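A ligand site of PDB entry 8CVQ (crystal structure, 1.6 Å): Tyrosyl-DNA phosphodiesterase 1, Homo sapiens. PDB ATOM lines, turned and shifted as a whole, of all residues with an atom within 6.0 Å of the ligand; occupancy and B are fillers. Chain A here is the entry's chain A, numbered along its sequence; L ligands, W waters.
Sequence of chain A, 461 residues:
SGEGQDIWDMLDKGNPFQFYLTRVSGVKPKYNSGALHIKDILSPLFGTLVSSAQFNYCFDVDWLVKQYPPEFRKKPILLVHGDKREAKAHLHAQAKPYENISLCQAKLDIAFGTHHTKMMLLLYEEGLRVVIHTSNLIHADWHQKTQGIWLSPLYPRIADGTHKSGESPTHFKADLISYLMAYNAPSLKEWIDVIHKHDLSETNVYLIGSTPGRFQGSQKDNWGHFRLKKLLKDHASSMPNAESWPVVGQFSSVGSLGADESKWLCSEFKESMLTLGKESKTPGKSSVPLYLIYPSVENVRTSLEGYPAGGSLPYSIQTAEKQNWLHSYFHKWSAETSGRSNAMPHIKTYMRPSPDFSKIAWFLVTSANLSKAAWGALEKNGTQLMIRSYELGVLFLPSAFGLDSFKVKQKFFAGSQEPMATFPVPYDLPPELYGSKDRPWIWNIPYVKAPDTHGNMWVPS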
ATOM      1  N   ASN A  56      -8.043  13.240   3.226  1.00  0.00           N
ATOM      2  CA  ASN A  56      -6.946  13.126   4.179  1.00  0.00           C
ATOM      3  C   ASN A  56      -7.485  12.819   5.566  1.00  0.00           C
ATOM      4  O   ASN A  56      -8.688  12.651   5.782  1.00  0.00           O
ATOM      5  CB  ASN A  56      -6.077  14.388   4.180  1.00  0.00           C
ATOM      6  CG  ASN A  56      -4.588  14.061   4.317  1.00  0.00           C
ATOM      7  OD1 ASN A  56      -4.165  13.610   5.365  1.00  0.00           O
ATOM      8  ND2 ASN A  56      -3.815  14.237   3.245  1.00  0.00           N
ATOM      9  N   TYR A  57      -6.548  12.764   6.519  1.00  0.00           N
ATOM     10  CA  TYR A  57      -6.860  12.565   7.929  1.00  0.00           C
ATOM     11  C   TYR A  57      -6.890  13.894   8.670  1.00  0.00           C
ATOM     12  O   TYR A  57      -7.894  14.237   9.308  1.00  0.00           O
ATOM     13  CB  TYR A  57      -5.846  11.599   8.565  1.00  0.00           C
ATOM     14  CG  TYR A  57      -5.995  11.589  10.065  1.00  0.00           C
ATOM     15  CD1 TYR A  57      -7.090  10.994  10.662  1.00  0.00           C
ATOM     16  CD2 TYR A  57      -5.056  12.226  10.887  1.00  0.00           C
ATOM     17  CE1 TYR A  57      -7.256  11.013  12.033  1.00  0.00           C
ATOM     18  CE2 TYR A  57      -5.217  12.258  12.256  1.00  0.00           C
ATOM     19  CZ  TYR A  57      -6.322  11.642  12.820  1.00  0.00           C
ATOM     20  OH  TYR A  57      -6.488  11.661  14.190  1.00  0.00           O
ATOM     21  N   PHE A 112     -14.074   2.841  16.332  1.00  0.00           N
ATOM     22  CA  PHE A 112     -12.612   2.906  16.329  1.00  0.00           C
ATOM     23  C   PHE A 112     -12.021   2.898  14.927  1.00  0.00           C
ATOM     24  O   PHE A 112     -10.886   2.443  14.725  1.00  0.00           O
ATOM     25  CB  PHE A 112     -12.011   1.789  17.198  1.00  0.00           C
ATOM     26  CG  PHE A 112     -12.566   1.757  18.610  1.00  0.00           C
ATOM     27  CD1 PHE A 112     -12.295   2.786  19.491  1.00  0.00           C
ATOM     28  CD2 PHE A 112     -13.363   0.707  19.039  1.00  0.00           C
ATOM     29  CE1 PHE A 112     -12.795   2.775  20.794  1.00  0.00           C
ATOM     30  CE2 PHE A 112     -13.869   0.683  20.342  1.00  0.00           C
ATOM     31  CZ  PHE A 112     -13.584   1.719  21.209  1.00  0.00           C
ATOM     32  N   GLY A 113     -12.771   3.404  13.946  1.00  0.00           N
ATOM     33  CA  GLY A 113     -12.276   3.570  12.605  1.00  0.00           C
ATOM     34  C   GLY A 113     -11.788   4.980  12.343  1.00  0.00           C
ATOM     35  O   GLY A 113     -12.127   5.926  13.054  1.00  0.00           O
ATOM     36  N   THR A 114     -10.978   5.117  11.295  1.00  0.00           N
ATOM     37  CA  THR A 114     -10.329   6.374  10.933  1.00  0.00           C
ATOM     38  C   THR A 114     -10.423   6.574   9.426  1.00  0.00           C
ATOM     39  O   THR A 114     -10.335   5.607   8.659  1.00  0.00           O
ATOM     40  CB  THR A 114      -8.853   6.356  11.347  1.00  0.00           C
ATOM     41  OG1 THR A 114      -8.767   6.113  12.750  1.00  0.00           O
ATOM     42  CG2 THR A 114      -8.173   7.679  11.008  1.00  0.00           C
ATOM     43  N   HIS A 115     -10.568   7.826   8.991  1.00  0.00           N
ATOM     44  CA  HIS A 115     -10.423   8.117   7.565  1.00  0.00           C
ATOM     45  C   HIS A 115      -8.960   8.465   7.295  1.00  0.00           C
ATOM     46  O   HIS A 115      -8.548   9.620   7.414  1.00  0.00           O
ATOM     47  CB  HIS A 115     -11.367   9.237   7.115  1.00  0.00           C
ATOM     48  CG  HIS A 115     -11.316   9.490   5.637  1.00  0.00           C
ATOM     49  ND1 HIS A 115     -10.448  10.404   5.073  1.00  0.00           N
ATOM     50  CD2 HIS A 115     -11.994   8.935   4.605  1.00  0.00           C
ATOM     51  CE1 HIS A 115     -10.603  10.404   3.758  1.00  0.00           C
ATOM     52  NE2 HIS A 115     -11.540   9.518   3.457  1.00  0.00           N
ATOM     53  N   HIS A 116      -8.174   7.441   6.927  1.00  0.00           N
ATOM     54  CA  HIS A 116      -6.727   7.590   6.720  1.00  0.00           C
ATOM     55  C   HIS A 116      -6.341   7.925   5.285  1.00  0.00           C
ATOM     56  O   HIS A 116      -5.218   8.396   5.065  1.00  0.00           O
ATOM     57  CB  HIS A 116      -5.956   6.307   7.057  1.00  0.00           C
ATOM     58  CG  HIS A 116      -5.715   6.066   8.507  1.00  0.00           C
ATOM     59  ND1 HIS A 116      -4.885   6.851   9.286  1.00  0.00           N
ATOM     60  CD2 HIS A 116      -6.151   5.065   9.321  1.00  0.00           C
ATOM     61  CE1 HIS A 116      -4.843   6.365  10.508  1.00  0.00           C
ATOM     62  NE2 HIS A 116      -5.607   5.285  10.556  1.00  0.00           N
ATOM     63  N   LYS A 118      -5.224   9.234   1.840  1.00  0.00           N
ATOM     64  CA  LYS A 118      -4.612  10.479   1.402  1.00  0.00           C
ATOM     65  C   LYS A 118      -4.555  10.460  -0.115  1.00  0.00           C
ATOM     66  O   LYS A 118      -3.822   9.676  -0.710  1.00  0.00           O
ATOM     67  CB  LYS A 118      -3.241  10.645   2.054  1.00  0.00           C
ATOM     68  CG  LYS A 118      -3.449  10.696   3.579  1.00  0.00           C
ATOM     69  CD  LYS A 118      -2.171  10.781   4.345  1.00  0.00           C
ATOM     70  CE  LYS A 118      -2.461  10.750   5.842  1.00  0.00           C
ATOM     71  NZ  LYS A 118      -2.888   9.404   6.283  1.00  0.00           N
ATOM     72  N   THR A 134       0.981   9.799   1.034  1.00  0.00           N
ATOM     73  CA  THR A 134       0.966   9.384   2.437  1.00  0.00           C
ATOM     74  C   THR A 134       0.991  10.528   3.438  1.00  0.00           C
ATOM     75  O   THR A 134       0.997  10.251   4.640  1.00  0.00           O
ATOM     76  CB  THR A 134       2.146   8.439   2.742  1.00  0.00           C
ATOM     77  OG1 THR A 134       3.390   9.150   2.609  1.00  0.00           O
ATOM     78  CG2 THR A 134       2.155   7.251   1.772  1.00  0.00           C
ATOM     79  N   ASN A 136      -0.237  13.866   5.618  1.00  0.00           N
ATOM     80  CA  ASN A 136      -1.281  14.783   6.070  1.00  0.00           C
ATOM     81  C   ASN A 136      -1.063  16.175   5.482  1.00  0.00           C
ATOM     82  O   ASN A 136       0.041  16.531   5.071  1.00  0.00           O
ATOM     83  CB  ASN A 136      -1.300  14.865   7.610  1.00  0.00           C
ATOM     84  CG  ASN A 136      -1.774  13.563   8.240  1.00  0.00           C
ATOM     85  OD1 ASN A 136      -2.969  13.291   8.286  1.00  0.00           O
ATOM     86  ND2 ASN A 136      -0.838  12.736   8.706  1.00  0.00           N
ATOM     87  N   ASP A 141       4.208  17.370   7.924  1.00  0.00           N
ATOM     88  CA  ASP A 141       4.276  16.124   7.169  1.00  0.00           C
ATOM     89  C   ASP A 141       5.065  16.259   5.873  1.00  0.00           C
ATOM     90  O   ASP A 141       5.490  15.239   5.322  1.00  0.00           O
ATOM     91  CB  ASP A 141       2.861  15.607   6.861  1.00  0.00           C
ATOM     92  CG  ASP A 141       2.374  14.642   7.922  1.00  0.00           C
ATOM     93  OD1 ASP A 141       2.572  14.948   9.124  1.00  0.00           O
ATOM     94  OD2 ASP A 141       1.817  13.576   7.581  1.00  0.00           O
ATOM     95  N   SER A 252       4.059   3.451  10.063  1.00  0.00           N
ATOM     96  CA  SER A 252       4.252   4.481  11.089  1.00  0.00           C
ATOM     97  C   SER A 252       3.362   4.316  12.312  1.00  0.00           C
ATOM     98  O   SER A 252       3.494   5.094  13.263  1.00  0.00           O
ATOM     99  CB  SER A 252       4.074   5.873  10.461  1.00  0.00           C
ATOM    100  OG  SER A 252       2.778   6.039   9.899  1.00  0.00           O
ATOM    101  N   SER A 253       2.482   3.319  12.342  1.00  0.00           N
ATOM    102  CA  SER A 253       1.584   3.135  13.467  1.00  0.00           C
ATOM    103  C   SER A 253       1.292   1.648  13.594  1.00  0.00           C
ATOM    104  O   SER A 253       1.319   0.902  12.609  1.00  0.00           O
ATOM    105  CB  SER A 253       0.296   3.942  13.266  1.00  0.00           C
ATOM    106  OG  SER A 253      -0.513   3.953  14.418  1.00  0.00           O
ATOM    107  N   GLY A 311       5.636  12.325  17.550  1.00  0.00           N
ATOM    108  CA  GLY A 311       4.228  12.710  17.543  1.00  0.00           C
ATOM    109  C   GLY A 311       3.460  12.222  16.331  1.00  0.00           C
ATOM    110  O   GLY A 311       2.230  12.231  16.359  1.00  0.00           O
ATOM    111  N   SER A 312       4.171  11.811  15.279  1.00  0.00           N
ATOM    112  CA  SER A 312       3.567  11.224  14.078  1.00  0.00           C
ATOM    113  C   SER A 312       3.899   9.747  13.928  1.00  0.00           C
ATOM    114  O   SER A 312       3.798   9.199  12.811  1.00  0.00           O
ATOM    115  CB  SER A 312       3.988  11.994  12.825  1.00  0.00           C
ATOM    116  OG  SER A 312       3.683  13.364  12.954  1.00  0.00           O
ATOM    117  N   LEU A 313       4.303   9.090  15.019  1.00  0.00           N
ATOM    118  CA  LEU A 313       4.551   7.649  15.052  1.00  0.00           C
ATOM    119  C   LEU A 313       3.671   7.097  16.173  1.00  0.00           C
ATOM    120  O   LEU A 313       4.154   6.828  17.293  1.00  0.00           O
ATOM    121  CB  LEU A 313       6.027   7.342  15.265  1.00  0.00           C
ATOM    122  CG  LEU A 313       6.932   7.731  14.091  1.00  0.00           C
ATOM    123  CD1 LEU A 313       8.390   7.817  14.541  1.00  0.00           C
ATOM    124  CD2 LEU A 313       6.796   6.727  12.935  1.00  0.00           C
ATOM    125  N   PRO A 314       2.363   6.957  15.922  1.00  0.00           N
ATOM    126  CA  PRO A 314       1.423   6.633  17.015  1.00  0.00           C
ATOM    127  C   PRO A 314       1.429   5.151  17.376  1.00  0.00           C
ATOM    128  O   PRO A 314       0.857   4.307  16.673  1.00  0.00           O
ATOM    129  CB  PRO A 314       0.061   7.063  16.451  1.00  0.00           C
ATOM    130  CG  PRO A 314       0.399   7.989  15.289  1.00  0.00           C
ATOM    131  CD  PRO A 314       1.641   7.353  14.708  1.00  0.00           C
ATOM    132  N   HIS A 346       6.731   8.450   7.469  1.00  0.00           N
ATOM    133  CA  HIS A 346       5.276   8.425   7.533  1.00  0.00           C
ATOM    134  C   HIS A 346       4.693   7.740   6.303  1.00  0.00           C
ATOM    135  O   HIS A 346       3.487   7.513   6.247  1.00  0.00           O
ATOM    136  CB  HIS A 346       4.734   9.855   7.727  1.00  0.00           C
ATOM    137  CG  HIS A 346       3.266   9.925   8.033  1.00  0.00           C
ATOM    138  ND1 HIS A 346       2.325  10.160   7.061  1.00  0.00           N
ATOM    139  CD2 HIS A 346       2.589   9.814   9.204  1.00  0.00           C
ATOM    140  CE1 HIS A 346       1.119  10.183   7.612  1.00  0.00           C
ATOM    141  NE2 HIS A 346       1.251   9.965   8.906  1.00  0.00           N
ATOM    142  N   LYS A 348       3.968   4.373   4.184  1.00  0.00           N
ATOM    143  CA  LYS A 348       3.752   2.957   4.475  1.00  0.00           C
ATOM    144  C   LYS A 348       3.989   2.208   3.194  1.00  0.00           C
ATOM    145  O   LYS A 348       3.523   2.638   2.127  1.00  0.00           O
ATOM    146  CB  LYS A 348       2.337   2.644   4.990  1.00  0.00           C
ATOM    147  CG  LYS A 348       1.987   3.292   6.323  1.00  0.00           C
ATOM    148  CD  LYS A 348       1.592   4.746   6.100  1.00  0.00           C
ATOM    149  CE  LYS A 348       0.921   5.316   7.318  1.00  0.00           C
ATOM    150  NZ  LYS A 348       1.158   6.760   7.414  1.00  0.00           N
ATOM    151  N   SER A 367      -1.704   4.088   2.627  1.00  0.00           N
ATOM    152  CA  SER A 367      -1.942   4.691   3.939  1.00  0.00           C
ATOM    153  C   SER A 367      -2.027   3.645   5.046  1.00  0.00           C
ATOM    154  O   SER A 367      -1.989   4.031   6.224  1.00  0.00           O
ATOM    155  CB  SER A 367      -3.248   5.488   3.909  1.00  0.00           C
ATOM    156  OG  SER A 367      -4.344   4.614   3.624  1.00  0.00           O
ATOM    157  N   ASN A 369      -1.494   1.221   7.882  1.00  0.00           N
ATOM    158  CA  ASN A 369      -0.533   0.839   8.906  1.00  0.00           C
ATOM    159  C   ASN A 369      -0.695  -0.626   9.284  1.00  0.00           C
ATOM    160  O   ASN A 369      -1.518  -1.366   8.729  1.00  0.00           O
ATOM    161  CB  ASN A 369      -0.694   1.750  10.118  1.00  0.00           C
ATOM    162  CG  ASN A 369      -0.102   3.098   9.886  1.00  0.00           C
ATOM    163  OD1 ASN A 369       1.101   3.219   9.659  1.00  0.00           O
ATOM    164  ND2 ASN A 369      -0.941   4.143   9.893  1.00  0.00           N
ATOM    165  N   TRP A 443       4.852   6.362  21.795  1.00  0.00           N
ATOM    166  CA  TRP A 443       4.763   7.813  21.735  1.00  0.00           C
ATOM    167  C   TRP A 443       4.316   8.464  23.035  1.00  0.00           C
ATOM    168  O   TRP A 443       4.563   9.668  23.211  1.00  0.00           O
ATOM    169  CB  TRP A 443       3.855   8.260  20.571  1.00  0.00           C
ATOM    170  CG  TRP A 443       2.361   8.081  20.724  1.00  0.00           C
ATOM    171  CD1 TRP A 443       1.702   7.241  21.583  1.00  0.00           C
ATOM    172  CD2 TRP A 443       1.352   8.771  19.979  1.00  0.00           C
ATOM    173  NE1 TRP A 443       0.334   7.378  21.421  1.00  0.00           N
ATOM    174  CE2 TRP A 443       0.099   8.308  20.436  1.00  0.00           C
ATOM    175  CE3 TRP A 443       1.388   9.737  18.963  1.00  0.00           C
ATOM    176  CZ2 TRP A 443      -1.116   8.792  19.928  1.00  0.00           C
ATOM    177  CZ3 TRP A 443       0.182  10.217  18.456  1.00  0.00           C
ATOM    178  CH2 TRP A 443      -1.043   9.744  18.941  1.00  0.00           C
HETATM  179  C1  LIG L   1      -4.542   9.356  16.426  1.00  0.00           C
HETATM  180  C2  LIG L   1      -3.420  12.749  17.321  1.00  0.00           C
HETATM  181  C3  LIG L   1      -1.978  11.886  15.602  1.00  0.00           C
HETATM  182  C4  LIG L   1      -6.835   5.503  17.212  1.00  0.00           C
HETATM  183  C5  LIG L   1      -7.430   4.467  17.926  1.00  0.00           C
HETATM  184  C6  LIG L   1      -7.486   3.193  17.382  1.00  0.00           C
HETATM  185  C7  LIG L   1      -8.574   2.373  19.354  1.00  0.00           C
HETATM  186  C8  LIG L   1      -7.944   4.686  19.192  1.00  0.00           C
HETATM  187  C9  LIG L   1      -6.252   6.564  15.135  1.00  0.00           C
HETATM  188  C10 LIG L   1      -0.499   7.208  10.648  1.00  0.00           C
HETATM  189  C11 LIG L   1      -1.655   7.678  11.516  1.00  0.00           C
HETATM  190  C12 LIG L   1      -1.818   7.108  12.770  1.00  0.00           C
HETATM  191  C13 LIG L   1      -2.875   7.527  13.568  1.00  0.00           C
HETATM  192  C14 LIG L   1      -3.746   8.495  13.105  1.00  0.00           C
HETATM  193  C15 LIG L   1      -4.997   8.637  15.322  1.00  0.00           C
HETATM  194  C16 LIG L   1      -3.813  10.550  16.428  1.00  0.00           C
HETATM  195  C17 LIG L   1      -4.161  11.576  17.304  1.00  0.00           C
HETATM  196  C18 LIG L   1      -2.338  12.909  16.470  1.00  0.00           C
HETATM  197  C19 LIG L   1      -2.718  10.712  15.584  1.00  0.00           C
HETATM  198  C20 LIG L   1      -5.588   7.581  17.108  1.00  0.00           C
HETATM  199  C21 LIG L   1      -6.190   6.552  17.864  1.00  0.00           C
HETATM  200  C22 LIG L   1      -8.050   2.150  18.088  1.00  0.00           C
HETATM  201  C23 LIG L   1      -8.521   3.641  19.906  1.00  0.00           C
HETATM  202  C24 LIG L   1      -6.862   5.517  15.822  1.00  0.00           C
HETATM  203  C25 LIG L   1      -3.565   9.056  11.851  1.00  0.00           C
HETATM  204  C26 LIG L   1      -2.538   8.643  11.047  1.00  0.00           C
HETATM  205  C27 LIG L   1      -2.403   9.294   9.674  1.00  0.00           C
HETATM  206  N1  LIG L   1      -4.852   8.977  13.921  1.00  0.00           N
HETATM  207  N2  LIG L   1      -4.919   8.677  17.501  1.00  0.00           N
HETATM  208  N3  LIG L   1      -5.633   7.555  15.799  1.00  0.00           N
HETATM  209  O1  LIG L   1       0.607   7.012  11.196  1.00  0.00           O
HETATM  210  O2  LIG L   1      -0.651   7.050   9.422  1.00  0.00           O
HETATM  211  O3  LIG L   1      -1.376   9.962   9.400  1.00  0.00           O
HETATM  212  O4  LIG L   1      -3.330   9.182   8.831  1.00  0.00           O
HETATM  213  O   HOH W   1      -6.674   0.132  15.795  1.00  0.00           O
HETATM  214  O   HOH W   2      -4.779   9.239  20.246  1.00  0.00           O
HETATM  215  O   HOH W   3      -2.337   6.702   7.159  1.00  0.00           O
HETATM  216  O   HOH W   4      -5.577  14.220  15.161  1.00  0.00           O
HETATM  217  O   HOH W   5      -8.112   9.887  15.559  1.00  0.00           O
HETATM  218  O   HOH W   6      -9.351   8.001  14.573  1.00  0.00           O
HETATM  219  O   HOH W   7      -9.255   0.267  15.634  1.00  0.00           O
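O4 of the ligand lies within salt-bridge range of NZ of Lys 118, 2.6 Å away. A ring nitrogen (NE2) of His 346 sits at hydrogen-bond distance from an oxygen (O3) of the ligand (2.7 Å). An oxygen (O1) of the ligand is in hydrogen-bond range of the side-chain hydroxyl (OG) of Ser 252 (2.7 Å). NZ of Lys 348 is in salt-bridge range of O2 of the ligand (2.7 Å). A ring nitrogen (ND1) of His 116 lies within hydrogen-bond range of an oxygen (O4) of the ligand, 2.8 Å away. The side-chain amide nitrogen of Asn 136 is in hydrogen-bond range of an oxygen (O3) of the ligand (2.9 Å). The side-chain amide nitrogen (ND2) of Asn 369 lies within hydrogen-bond range of an oxygen (O2) of the ligand. OH of Tyr 57 is in hydrogen-bond range of N1 of the ligand.
The side-chain amino group of Lys 118 lies within hydrogen-bond range of the backbone carbonyl oxygen of His 116, 2.8 Å away. The backbone carbonyl oxygen of His 346 sits at hydrogen-bond distance from the side-chain amino group of Lys 348, 2.7 Å away. The side-chain amide nitrogen of Asn 136 sits close to a ring nitrogen (NE2) of His 346, 3.5 Å away. A ring nitrogen (ND1) of His 346 sits at hydrogen-bond distance from the backbone carbonyl oxygen (O) of Thr 134, at 2.8 Å. The side-chain hydroxyl (OG) of Ser 252 sits at hydrogen-bond distance from the side-chain amino group (NZ) of Lys 348, 3.1 Å away. The backbone NH (N) of Ser 252 lies within hydrogen-bond range of the side-chain amide oxygen (OD1) of Asn 369, at 3.0 Å. The backbone NH of Ser 253 sits at hydrogen-bond distance from the side-chain amide oxygen of Asn 369 (3.0 Å). O of Pro 314 sits at hydrogen-bond distance from OG of Ser 253 (2.7 Å).
CD1 of Phe 112 touches C7 of the ligand (3.7 Å). OG1 of Thr 114 touches C9 of the ligand, at 3.5 Å. Ser 253 touches the ligand (CB to O1, 3.7 Å). Pro 314 touches the ligand. Trp 443 touches the ligand (CH2 to C16, 3.8 Å). Hydrophobic or aromatic side chains that line the ligand: Tyr 57, Phe 112, His 116, Pro 314, His 346 and Trp 443. Along chain A the residues within 4 Å of the ligand span positions 57 to 443.
Water W3 lies within hydrogen-bond range of O2 of the ligand (2.8 Å), O of Ser 367 (2.9 Å), NZ of Lys 118 (2.9 Å) and ND1 of His 116 (3.3 Å).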
